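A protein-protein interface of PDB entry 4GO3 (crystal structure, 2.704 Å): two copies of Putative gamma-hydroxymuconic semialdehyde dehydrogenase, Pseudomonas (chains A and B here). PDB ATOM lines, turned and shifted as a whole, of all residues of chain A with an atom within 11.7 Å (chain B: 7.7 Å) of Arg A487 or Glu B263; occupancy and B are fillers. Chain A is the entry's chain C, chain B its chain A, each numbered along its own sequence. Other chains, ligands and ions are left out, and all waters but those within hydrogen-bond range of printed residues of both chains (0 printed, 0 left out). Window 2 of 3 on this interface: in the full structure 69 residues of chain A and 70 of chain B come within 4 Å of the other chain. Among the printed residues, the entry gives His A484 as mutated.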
ATOM      1  N   ASN A 476       2.745 -26.255   9.027  1.00  0.00           N
ATOM      2  CA  ASN A 476       2.074 -27.526   9.077  1.00  0.00           C
ATOM      3  C   ASN A 476       2.361 -28.255   7.810  1.00  0.00           C
ATOM      4  O   ASN A 476       1.664 -28.090   6.842  1.00  0.00           O
ATOM      5  CB  ASN A 476       0.579 -27.335   9.217  1.00  0.00           C
ATOM      6  CG  ASN A 476      -0.148 -28.622   9.389  1.00  0.00           C
ATOM      7  OD1 ASN A 476       0.428 -29.684   9.265  1.00  0.00           O
ATOM      8  ND2 ASN A 476      -1.420 -28.538   9.682  1.00  0.00           N
ATOM      9  N   ALA A 479       0.959 -32.863   8.804  1.00  0.00           N
ATOM     10  CA  ALA A 479       0.368 -33.090  10.113  1.00  0.00           C
ATOM     11  C   ALA A 479      -1.079 -33.557  10.074  1.00  0.00           C
ATOM     12  O   ALA A 479      -1.912 -32.999   9.367  1.00  0.00           O
ATOM     13  CB  ALA A 479       0.504 -31.862  10.969  1.00  0.00           C
ATOM     14  N   ILE A 481      -4.442 -33.538  11.542  1.00  0.00           N
ATOM     15  CA  ILE A 481      -5.126 -32.734  12.521  1.00  0.00           C
ATOM     16  C   ILE A 481      -6.618 -32.956  12.574  1.00  0.00           C
ATOM     17  O   ILE A 481      -7.379 -32.348  11.845  1.00  0.00           O
ATOM     18  CB  ILE A 481      -4.807 -31.255  12.359  1.00  0.00           C
ATOM     19  CG1 ILE A 481      -3.436 -31.081  11.741  1.00  0.00           C
ATOM     20  CG2 ILE A 481      -4.785 -30.568  13.702  1.00  0.00           C
ATOM     21  CD1 ILE A 481      -2.833 -29.767  12.063  1.00  0.00           C
ATOM     22  N   ALA A 482      -7.038 -33.826  13.469  1.00  0.00           N
ATOM     23  CA  ALA A 482      -8.447 -33.970  13.699  1.00  0.00           C
ATOM     24  C   ALA A 482      -8.992 -32.623  14.107  1.00  0.00           C
ATOM     25  O   ALA A 482      -8.467 -31.976  14.996  1.00  0.00           O
ATOM     26  CB  ALA A 482      -8.701 -34.987  14.786  1.00  0.00           C
ATOM     27  N   PRO A 483     -10.060 -32.209  13.454  1.00  0.00           N
ATOM     28  CA  PRO A 483     -10.802 -31.038  13.869  1.00  0.00           C
ATOM     29  C   PRO A 483     -11.137 -31.096  15.336  1.00  0.00           C
ATOM     30  O   PRO A 483     -11.395 -32.156  15.853  1.00  0.00           O
ATOM     31  CB  PRO A 483     -12.042 -31.151  13.016  1.00  0.00           C
ATOM     32  CG  PRO A 483     -11.494 -31.705  11.706  1.00  0.00           C
ATOM     33  CD  PRO A 483     -10.190 -32.392  12.008  1.00  0.00           C
ATOM     34  N   HIS A 484     -11.101 -29.954  16.001  1.00  0.00           N
ATOM     35  CA  HIS A 484     -11.312 -29.910  17.426  1.00  0.00           C
ATOM     36  C   HIS A 484     -12.737 -30.281  17.737  1.00  0.00           C
ATOM     37  O   HIS A 484     -13.037 -30.981  18.682  1.00  0.00           O
ATOM     38  CB  HIS A 484     -11.014 -28.516  17.934  1.00  0.00           C
ATOM     39  CG  HIS A 484     -11.136 -28.391  19.409  1.00  0.00           C
ATOM     40  ND1 HIS A 484     -12.003 -27.511  20.006  1.00  0.00           N
ATOM     41  CD2 HIS A 484     -10.520 -29.055  20.409  1.00  0.00           C
ATOM     42  CE1 HIS A 484     -11.910 -27.630  21.314  1.00  0.00           C
ATOM     43  NE2 HIS A 484     -11.018 -28.562  21.584  1.00  0.00           N
ATOM     44  N   PHE A 485     -13.595 -29.757  16.901  1.00  0.00           N
ATOM     45  CA  PHE A 485     -15.002 -30.016  16.770  1.00  0.00           C
ATOM     46  C   PHE A 485     -15.175 -31.029  15.681  1.00  0.00           C
ATOM     47  O   PHE A 485     -15.336 -30.677  14.536  1.00  0.00           O
ATOM     48  CB  PHE A 485     -15.712 -28.744  16.341  1.00  0.00           C
ATOM     49  CG  PHE A 485     -15.375 -27.574  17.181  1.00  0.00           C
ATOM     50  CD1 PHE A 485     -15.807 -27.505  18.482  1.00  0.00           C
ATOM     51  CD2 PHE A 485     -14.599 -26.550  16.687  1.00  0.00           C
ATOM     52  CE1 PHE A 485     -15.488 -26.439  19.263  1.00  0.00           C
ATOM     53  CE2 PHE A 485     -14.276 -25.482  17.468  1.00  0.00           C
ATOM     54  CZ  PHE A 485     -14.722 -25.426  18.754  1.00  0.00           C
ATOM     55  N   LYS A 486     -15.144 -32.303  16.039  1.00  0.00           N
ATOM     56  CA  LYS A 486     -15.379 -33.339  15.058  1.00  0.00           C
ATOM     57  C   LYS A 486     -16.575 -32.925  14.211  1.00  0.00           C
ATOM     58  O   LYS A 486     -17.649 -32.652  14.735  1.00  0.00           O
ATOM     59  CB  LYS A 486     -15.626 -34.669  15.754  1.00  0.00           C
ATOM     60  CG  LYS A 486     -14.698 -34.912  16.925  1.00  0.00           C
ATOM     61  CD  LYS A 486     -15.104 -36.146  17.700  1.00  0.00           C
ATOM     62  CE  LYS A 486     -14.447 -37.387  17.133  1.00  0.00           C
ATOM     63  NZ  LYS A 486     -14.112 -38.354  18.205  1.00  0.00           N
ATOM     64  N   ARG A 487     -16.373 -32.889  12.897  1.00  0.00           N
ATOM     65  CA  ARG A 487     -17.394 -32.441  11.961  1.00  0.00           C
ATOM     66  C   ARG A 487     -18.531 -31.723  12.677  1.00  0.00           C
ATOM     67  O   ARG A 487     -18.651 -30.499  12.601  1.00  0.00           O
ATOM     68  CB  ARG A 487     -17.924 -33.614  11.134  1.00  0.00           C
ATOM     69  CG  ARG A 487     -16.986 -34.048  10.018  1.00  0.00           C
ATOM     70  CD  ARG A 487     -17.735 -34.312   8.723  1.00  0.00           C
ATOM     71  NE  ARG A 487     -17.205 -33.535   7.606  1.00  0.00           N
ATOM     72  CZ  ARG A 487     -16.592 -34.060   6.548  1.00  0.00           C
ATOM     73  NH1 ARG A 487     -16.427 -35.372   6.457  1.00  0.00           N
ATOM     74  NH2 ARG A 487     -16.145 -33.273   5.578  1.00  0.00           N
ATOM     75  N   ALA B 260      -5.787 -21.484  -0.045  1.00  0.00           N
ATOM     76  CA  ALA B 260      -5.875 -22.262   1.166  1.00  0.00           C
ATOM     77  C   ALA B 260      -6.816 -23.406   1.018  1.00  0.00           C
ATOM     78  O   ALA B 260      -7.753 -23.326   0.307  1.00  0.00           O
ATOM     79  CB  ALA B 260      -6.311 -21.425   2.280  1.00  0.00           C
ATOM     80  N   ASN B 261      -6.537 -24.460   1.762  1.00  0.00           N
ATOM     81  CA  ASN B 261      -7.427 -25.584   1.932  1.00  0.00           C
ATOM     82  C   ASN B 261      -8.529 -25.176   2.879  1.00  0.00           C
ATOM     83  O   ASN B 261      -8.359 -25.175   4.085  1.00  0.00           O
ATOM     84  CB  ASN B 261      -6.650 -26.770   2.491  1.00  0.00           C
ATOM     85  CG  ASN B 261      -7.529 -27.914   2.867  1.00  0.00           C
ATOM     86  OD1 ASN B 261      -8.732 -27.781   2.921  1.00  0.00           O
ATOM     87  ND2 ASN B 261      -6.931 -29.045   3.132  1.00  0.00           N
ATOM     88  N   ILE B 262      -9.659 -24.805   2.306  1.00  0.00           N
ATOM     89  CA  ILE B 262     -10.697 -24.112   3.027  1.00  0.00           C
ATOM     90  C   ILE B 262     -11.430 -24.974   4.026  1.00  0.00           C
ATOM     91  O   ILE B 262     -11.973 -24.454   4.974  1.00  0.00           O
ATOM     92  CB  ILE B 262     -11.671 -23.408   2.080  1.00  0.00           C
ATOM     93  CG1 ILE B 262     -11.049 -22.134   1.543  1.00  0.00           C
ATOM     94  CG2 ILE B 262     -12.925 -23.056   2.807  1.00  0.00           C
ATOM     95  CD1 ILE B 262     -11.093 -22.048   0.096  1.00  0.00           C
ATOM     96  N   GLU B 263     -11.399 -26.280   3.891  1.00  0.00           N
ATOM     97  CA  GLU B 263     -11.964 -27.108   4.937  1.00  0.00           C
ATOM     98  C   GLU B 263     -11.042 -27.111   6.140  1.00  0.00           C
ATOM     99  O   GLU B 263     -11.478 -27.043   7.267  1.00  0.00           O
ATOM    100  CB  GLU B 263     -12.162 -28.528   4.441  1.00  0.00           C
ATOM    101  CG  GLU B 263     -13.242 -29.268   5.146  1.00  0.00           C
ATOM    102  CD  GLU B 263     -12.905 -30.704   5.305  1.00  0.00           C
ATOM    103  OE1 GLU B 263     -12.143 -31.210   4.473  1.00  0.00           O
ATOM    104  OE2 GLU B 263     -13.398 -31.323   6.261  1.00  0.00           O
ATOM    105  N   ALA B 264      -9.750 -27.195   5.874  1.00  0.00           N
ATOM    106  CA  ALA B 264      -8.744 -27.197   6.907  1.00  0.00           C
ATOM    107  C   ALA B 264      -8.734 -25.862   7.591  1.00  0.00           C
ATOM    108  O   ALA B 264      -8.708 -25.791   8.805  1.00  0.00           O
ATOM    109  CB  ALA B 264      -7.384 -27.494   6.315  1.00  0.00           C
ATOM    110  N   ALA B 265      -8.748 -24.802   6.796  1.00  0.00           N
ATOM    111  CA  ALA B 265      -8.720 -23.449   7.324  1.00  0.00           C
ATOM    112  C   ALA B 265      -9.917 -23.197   8.225  1.00  0.00           C
ATOM    113  O   ALA B 265      -9.789 -22.558   9.265  1.00  0.00           O
ATOM    114  CB  ALA B 265      -8.655 -22.422   6.192  1.00  0.00           C
ATOM    115  N   VAL B 266     -11.080 -23.697   7.828  1.00  0.00           N
ATOM    116  CA  VAL B 266     -12.287 -23.508   8.621  1.00  0.00           C
ATOM    117  C   VAL B 266     -12.163 -24.213   9.961  1.00  0.00           C
ATOM    118  O   VAL B 266     -12.443 -23.628  11.004  1.00  0.00           O
ATOM    119  CB  VAL B 266     -13.519 -24.027   7.907  1.00  0.00           C
ATOM    120  CG1 VAL B 266     -14.694 -24.034   8.862  1.00  0.00           C
ATOM    121  CG2 VAL B 266     -13.818 -23.163   6.689  1.00  0.00           C
ATOM    122  N   ASN B 267     -11.725 -25.457   9.952  1.00  0.00           N
ATOM    123  CA  ASN B 267     -11.504 -26.167  11.191  1.00  0.00           C
ATOM    124  C   ASN B 267     -10.475 -25.486  12.063  1.00  0.00           C
ATOM    125  O   ASN B 267     -10.654 -25.382  13.256  1.00  0.00           O
ATOM    126  CB  ASN B 267     -11.047 -27.577  10.911  1.00  0.00           C
ATOM    127  CG  ASN B 267     -12.143 -28.448  10.415  1.00  0.00           C
ATOM    128  OD1 ASN B 267     -13.287 -28.300  10.796  1.00  0.00           O
ATOM    129  ND2 ASN B 267     -11.798 -29.378   9.556  1.00  0.00           N
ATOM    130  N   GLY B 268      -9.389 -25.032  11.461  1.00  0.00           N
ATOM    131  CA  GLY B 268      -8.366 -24.327  12.199  1.00  0.00           C
ATOM    132  C   GLY B 268      -8.901 -23.047  12.797  1.00  0.00           C
ATOM    133  O   GLY B 268      -8.679 -22.766  13.986  1.00  0.00           O
ATOM    134  N   ALA B 269      -9.597 -22.265  11.977  1.00  0.00           N
ATOM    135  CA  ALA B 269     -10.168 -21.000  12.433  1.00  0.00           C
ATOM    136  C   ALA B 269     -11.161 -21.235  13.565  1.00  0.00           C
ATOM    137  O   ALA B 269     -11.198 -20.488  14.546  1.00  0.00           O
ATOM    138  CB  ALA B 269     -10.849 -20.284  11.304  1.00  0.00           C
ATOM    139  N   GLN B 296     -17.100 -18.895   0.209  1.00  0.00           N
ATOM    140  CA  GLN B 296     -16.992 -20.329   0.362  1.00  0.00           C
ATOM    141  C   GLN B 296     -16.652 -20.640   1.789  1.00  0.00           C
ATOM    142  O   GLN B 296     -17.203 -21.544   2.380  1.00  0.00           O
ATOM    143  CB  GLN B 296     -15.924 -20.892  -0.563  1.00  0.00           C
ATOM    144  CG  GLN B 296     -16.174 -20.556  -2.000  1.00  0.00           C
ATOM    145  CD  GLN B 296     -14.931 -20.160  -2.733  1.00  0.00           C
ATOM    146  OE1 GLN B 296     -14.039 -20.977  -2.942  1.00  0.00           O
ATOM    147  NE2 GLN B 296     -14.861 -18.900  -3.140  1.00  0.00           N
ATOM    148  N   PHE B 297     -15.739 -19.861   2.341  1.00  0.00           N
ATOM    149  CA  PHE B 297     -15.266 -20.086   3.686  1.00  0.00           C
ATOM    150  C   PHE B 297     -16.355 -19.891   4.703  1.00  0.00           C
ATOM    151  O   PHE B 297     -16.635 -20.785   5.481  1.00  0.00           O
ATOM    152  CB  PHE B 297     -14.126 -19.116   3.987  1.00  0.00           C
ATOM    153  CG  PHE B 297     -13.475 -19.327   5.324  1.00  0.00           C
ATOM    154  CD1 PHE B 297     -12.371 -20.125   5.449  1.00  0.00           C
ATOM    155  CD2 PHE B 297     -13.954 -18.707   6.441  1.00  0.00           C
ATOM    156  CE1 PHE B 297     -11.785 -20.308   6.656  1.00  0.00           C
ATOM    157  CE2 PHE B 297     -13.363 -18.893   7.636  1.00  0.00           C
ATOM    158  CZ  PHE B 297     -12.283 -19.693   7.745  1.00  0.00           C
ATOM    159  N   ARG B 300     -19.047 -22.537   5.461  1.00  0.00           N
ATOM    160  CA  ARG B 300     -18.782 -23.698   6.261  1.00  0.00           C
ATOM    161  C   ARG B 300     -18.437 -23.283   7.656  1.00  0.00           C
ATOM    162  O   ARG B 300     -18.669 -24.017   8.597  1.00  0.00           O
ATOM    163  CB  ARG B 300     -17.639 -24.491   5.659  1.00  0.00           C
ATOM    164  CG  ARG B 300     -17.419 -24.195   4.224  1.00  0.00           C
ATOM    165  CD  ARG B 300     -16.211 -24.907   3.708  1.00  0.00           C
ATOM    166  NE  ARG B 300     -16.332 -26.336   3.908  1.00  0.00           N
ATOM    167  CZ  ARG B 300     -15.733 -27.253   3.163  1.00  0.00           C
ATOM    168  NH1 ARG B 300     -14.962 -26.891   2.151  1.00  0.00           N
ATOM    169  NH2 ARG B 300     -15.911 -28.529   3.434  1.00  0.00           N
ATOM    170  N   ALA B 303     -21.686 -22.225   9.573  1.00  0.00           N
ATOM    171  CA  ALA B 303     -22.431 -23.413   9.892  1.00  0.00           C
ATOM    172  C   ALA B 303     -21.744 -24.147  11.020  1.00  0.00           C
ATOM    173  O   ALA B 303     -22.391 -24.709  11.894  1.00  0.00           O
ATOM    174  CB  ALA B 303     -22.523 -24.289   8.704  1.00  0.00           C
ATOM    175  N   LEU B 304     -20.431 -24.055  11.063  1.00  0.00           N
ATOM    176  CA  LEU B 304     -19.720 -24.640  12.168  1.00  0.00           C
ATOM    177  C   LEU B 304     -20.029 -23.882  13.446  1.00  0.00           C
ATOM    178  O   LEU B 304     -20.523 -24.439  14.409  1.00  0.00           O
ATOM    179  CB  LEU B 304     -18.229 -24.647  11.883  1.00  0.00           C
ATOM    180  CG  LEU B 304     -17.391 -25.542  12.773  1.00  0.00           C
ATOM    181  CD1 LEU B 304     -17.887 -26.942  12.741  1.00  0.00           C
ATOM    182  CD2 LEU B 304     -16.001 -25.478  12.283  1.00  0.00           C
ATOM    183  N   SER B 307     -23.044 -24.657  14.973  1.00  0.00           N
ATOM    184  CA  SER B 307     -23.247 -26.052  15.281  1.00  0.00           C
ATOM    185  C   SER B 307     -22.625 -26.380  16.601  1.00  0.00           C
ATOM    186  O   SER B 307     -22.793 -27.457  17.131  1.00  0.00           O
ATOM    187  CB  SER B 307     -22.590 -26.911  14.216  1.00  0.00           C
ATOM    188  OG  SER B 307     -21.216 -26.612  14.114  1.00  0.00           O
ATOM    189  N   ILE B 308     -21.881 -25.433  17.132  1.00  0.00           N
ATOM    190  CA  ILE B 308     -21.085 -25.702  18.310  1.00  0.00           C
ATOM    191  C   ILE B 308     -21.897 -25.887  19.581  1.00  0.00           C
ATOM    192  O   ILE B 308     -22.750 -25.079  19.928  1.00  0.00           O
ATOM    193  CB  ILE B 308     -19.979 -24.658  18.489  1.00  0.00           C
ATOM    194  CG1 ILE B 308     -18.820 -24.970  17.544  1.00  0.00           C
ATOM    195  CG2 ILE B 308     -19.496 -24.649  19.907  1.00  0.00           C
ATOM    196  CD1 ILE B 308     -18.115 -23.771  17.014  1.00  0.00           C
ATOM    197  N   GLU B 319     -18.893 -28.730  23.682  1.00  0.00           N
ATOM    198  CA  GLU B 319     -17.852 -28.282  22.799  1.00  0.00           C
ATOM    199  C   GLU B 319     -17.263 -26.974  23.273  1.00  0.00           C
ATOM    200  O   GLU B 319     -16.060 -26.797  23.259  1.00  0.00           O
ATOM    201  CB  GLU B 319     -18.425 -28.110  21.415  1.00  0.00           C
ATOM    202  CG  GLU B 319     -18.527 -29.368  20.654  1.00  0.00           C
ATOM    203  CD  GLU B 319     -19.232 -29.138  19.374  1.00  0.00           C
ATOM    204  OE1 GLU B 319     -20.358 -28.629  19.433  1.00  0.00           O
ATOM    205  OE2 GLU B 319     -18.667 -29.445  18.313  1.00  0.00           O
ATOM    206  N   TRP B 414      -3.072 -19.212   6.019  1.00  0.00           N
ATOM    207  CA  TRP B 414      -3.365 -20.448   5.329  1.00  0.00           C
ATOM    208  C   TRP B 414      -3.117 -20.276   3.846  1.00  0.00           C
ATOM    209  O   TRP B 414      -3.741 -19.458   3.185  1.00  0.00           O
ATOM    210  CB  TRP B 414      -4.793 -20.862   5.608  1.00  0.00           C
ATOM    211  CG  TRP B 414      -5.059 -21.032   7.073  1.00  0.00           C
ATOM    212  CD1 TRP B 414      -5.204 -20.047   8.001  1.00  0.00           C
ATOM    213  CD2 TRP B 414      -5.221 -22.269   7.774  1.00  0.00           C
ATOM    214  NE1 TRP B 414      -5.440 -20.591   9.244  1.00  0.00           N
ATOM    215  CE2 TRP B 414      -5.450 -21.956   9.132  1.00  0.00           C
ATOM    216  CE3 TRP B 414      -5.179 -23.613   7.390  1.00  0.00           C
ATOM    217  CZ2 TRP B 414      -5.641 -22.932  10.106  1.00  0.00           C
ATOM    218  CZ3 TRP B 414      -5.366 -24.584   8.360  1.00  0.00           C
ATOM    219  CH2 TRP B 414      -5.602 -24.234   9.707  1.00  0.00           C
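NH2 of Arg A487 lies within salt-bridge range of OE2 of Glu B263 (3.4 Å).
ND2 of Asn B267 is in hydrogen-bond range of O of Glu B263 (3.3 Å). N of Glu B263 sits at hydrogen-bond distance from OD1 of Asn B261.
Among the printed residues, merely in contact across the chains: Pro A483 with Asn B267, Phe A485 with Glu B319 and Arg A487 with Leu B304.
Ala A479 touches none of the printed residues of chain B. Printed residues of chain B within 4 Å of Pro A483: Asn B267 (3.2 Å). Printed residues of chain B within 4 Å of Phe A485: Glu B319 (3.5 Å). No residue of chain A comes within 4 Å of Asn B261. Glu B263 touches just one residue of chain A: Arg A487 (3.4 Å). No residue of chain A comes within 4 Å of Ala B265. Of chain A, only Pro A483 (3.2 Å) comes within 4 Å of Asn B267. Ala B303 touches none of the printed residues of chain A. Leu B304 touches just one residue of chain A: Arg A487. Of the printed residues of chain A, Glu B319 touches Phe A485 (3.5 Å). The nearest printed residue of chain B that does not touch Phe A485 is Ile B308 (4.03 Å).
Of the 19 printed residues of chain B, 4 touch a printed residue of chain A. Printed residues of chain B that touch a printed residue of chain A: Glu B263, Asn B267, Leu B304 and Glu B319. Hydrophobic or aromatic side chains of chain B within 4 Å of the printed part of chain A: Leu B304. Among the printed residues, 4 pairs touch across the chains. Among the printed residues, Asp or Glu carboxylates within 4 Å of a Lys or Arg side-chain nitrogen of the other chain: Arg A487 with Glu B263 (3.4 Å).
No position is printed for both chains. Of the 4 pairs that touch across the chains among the printed residues, none has its exchanged pair printed and touching as well.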
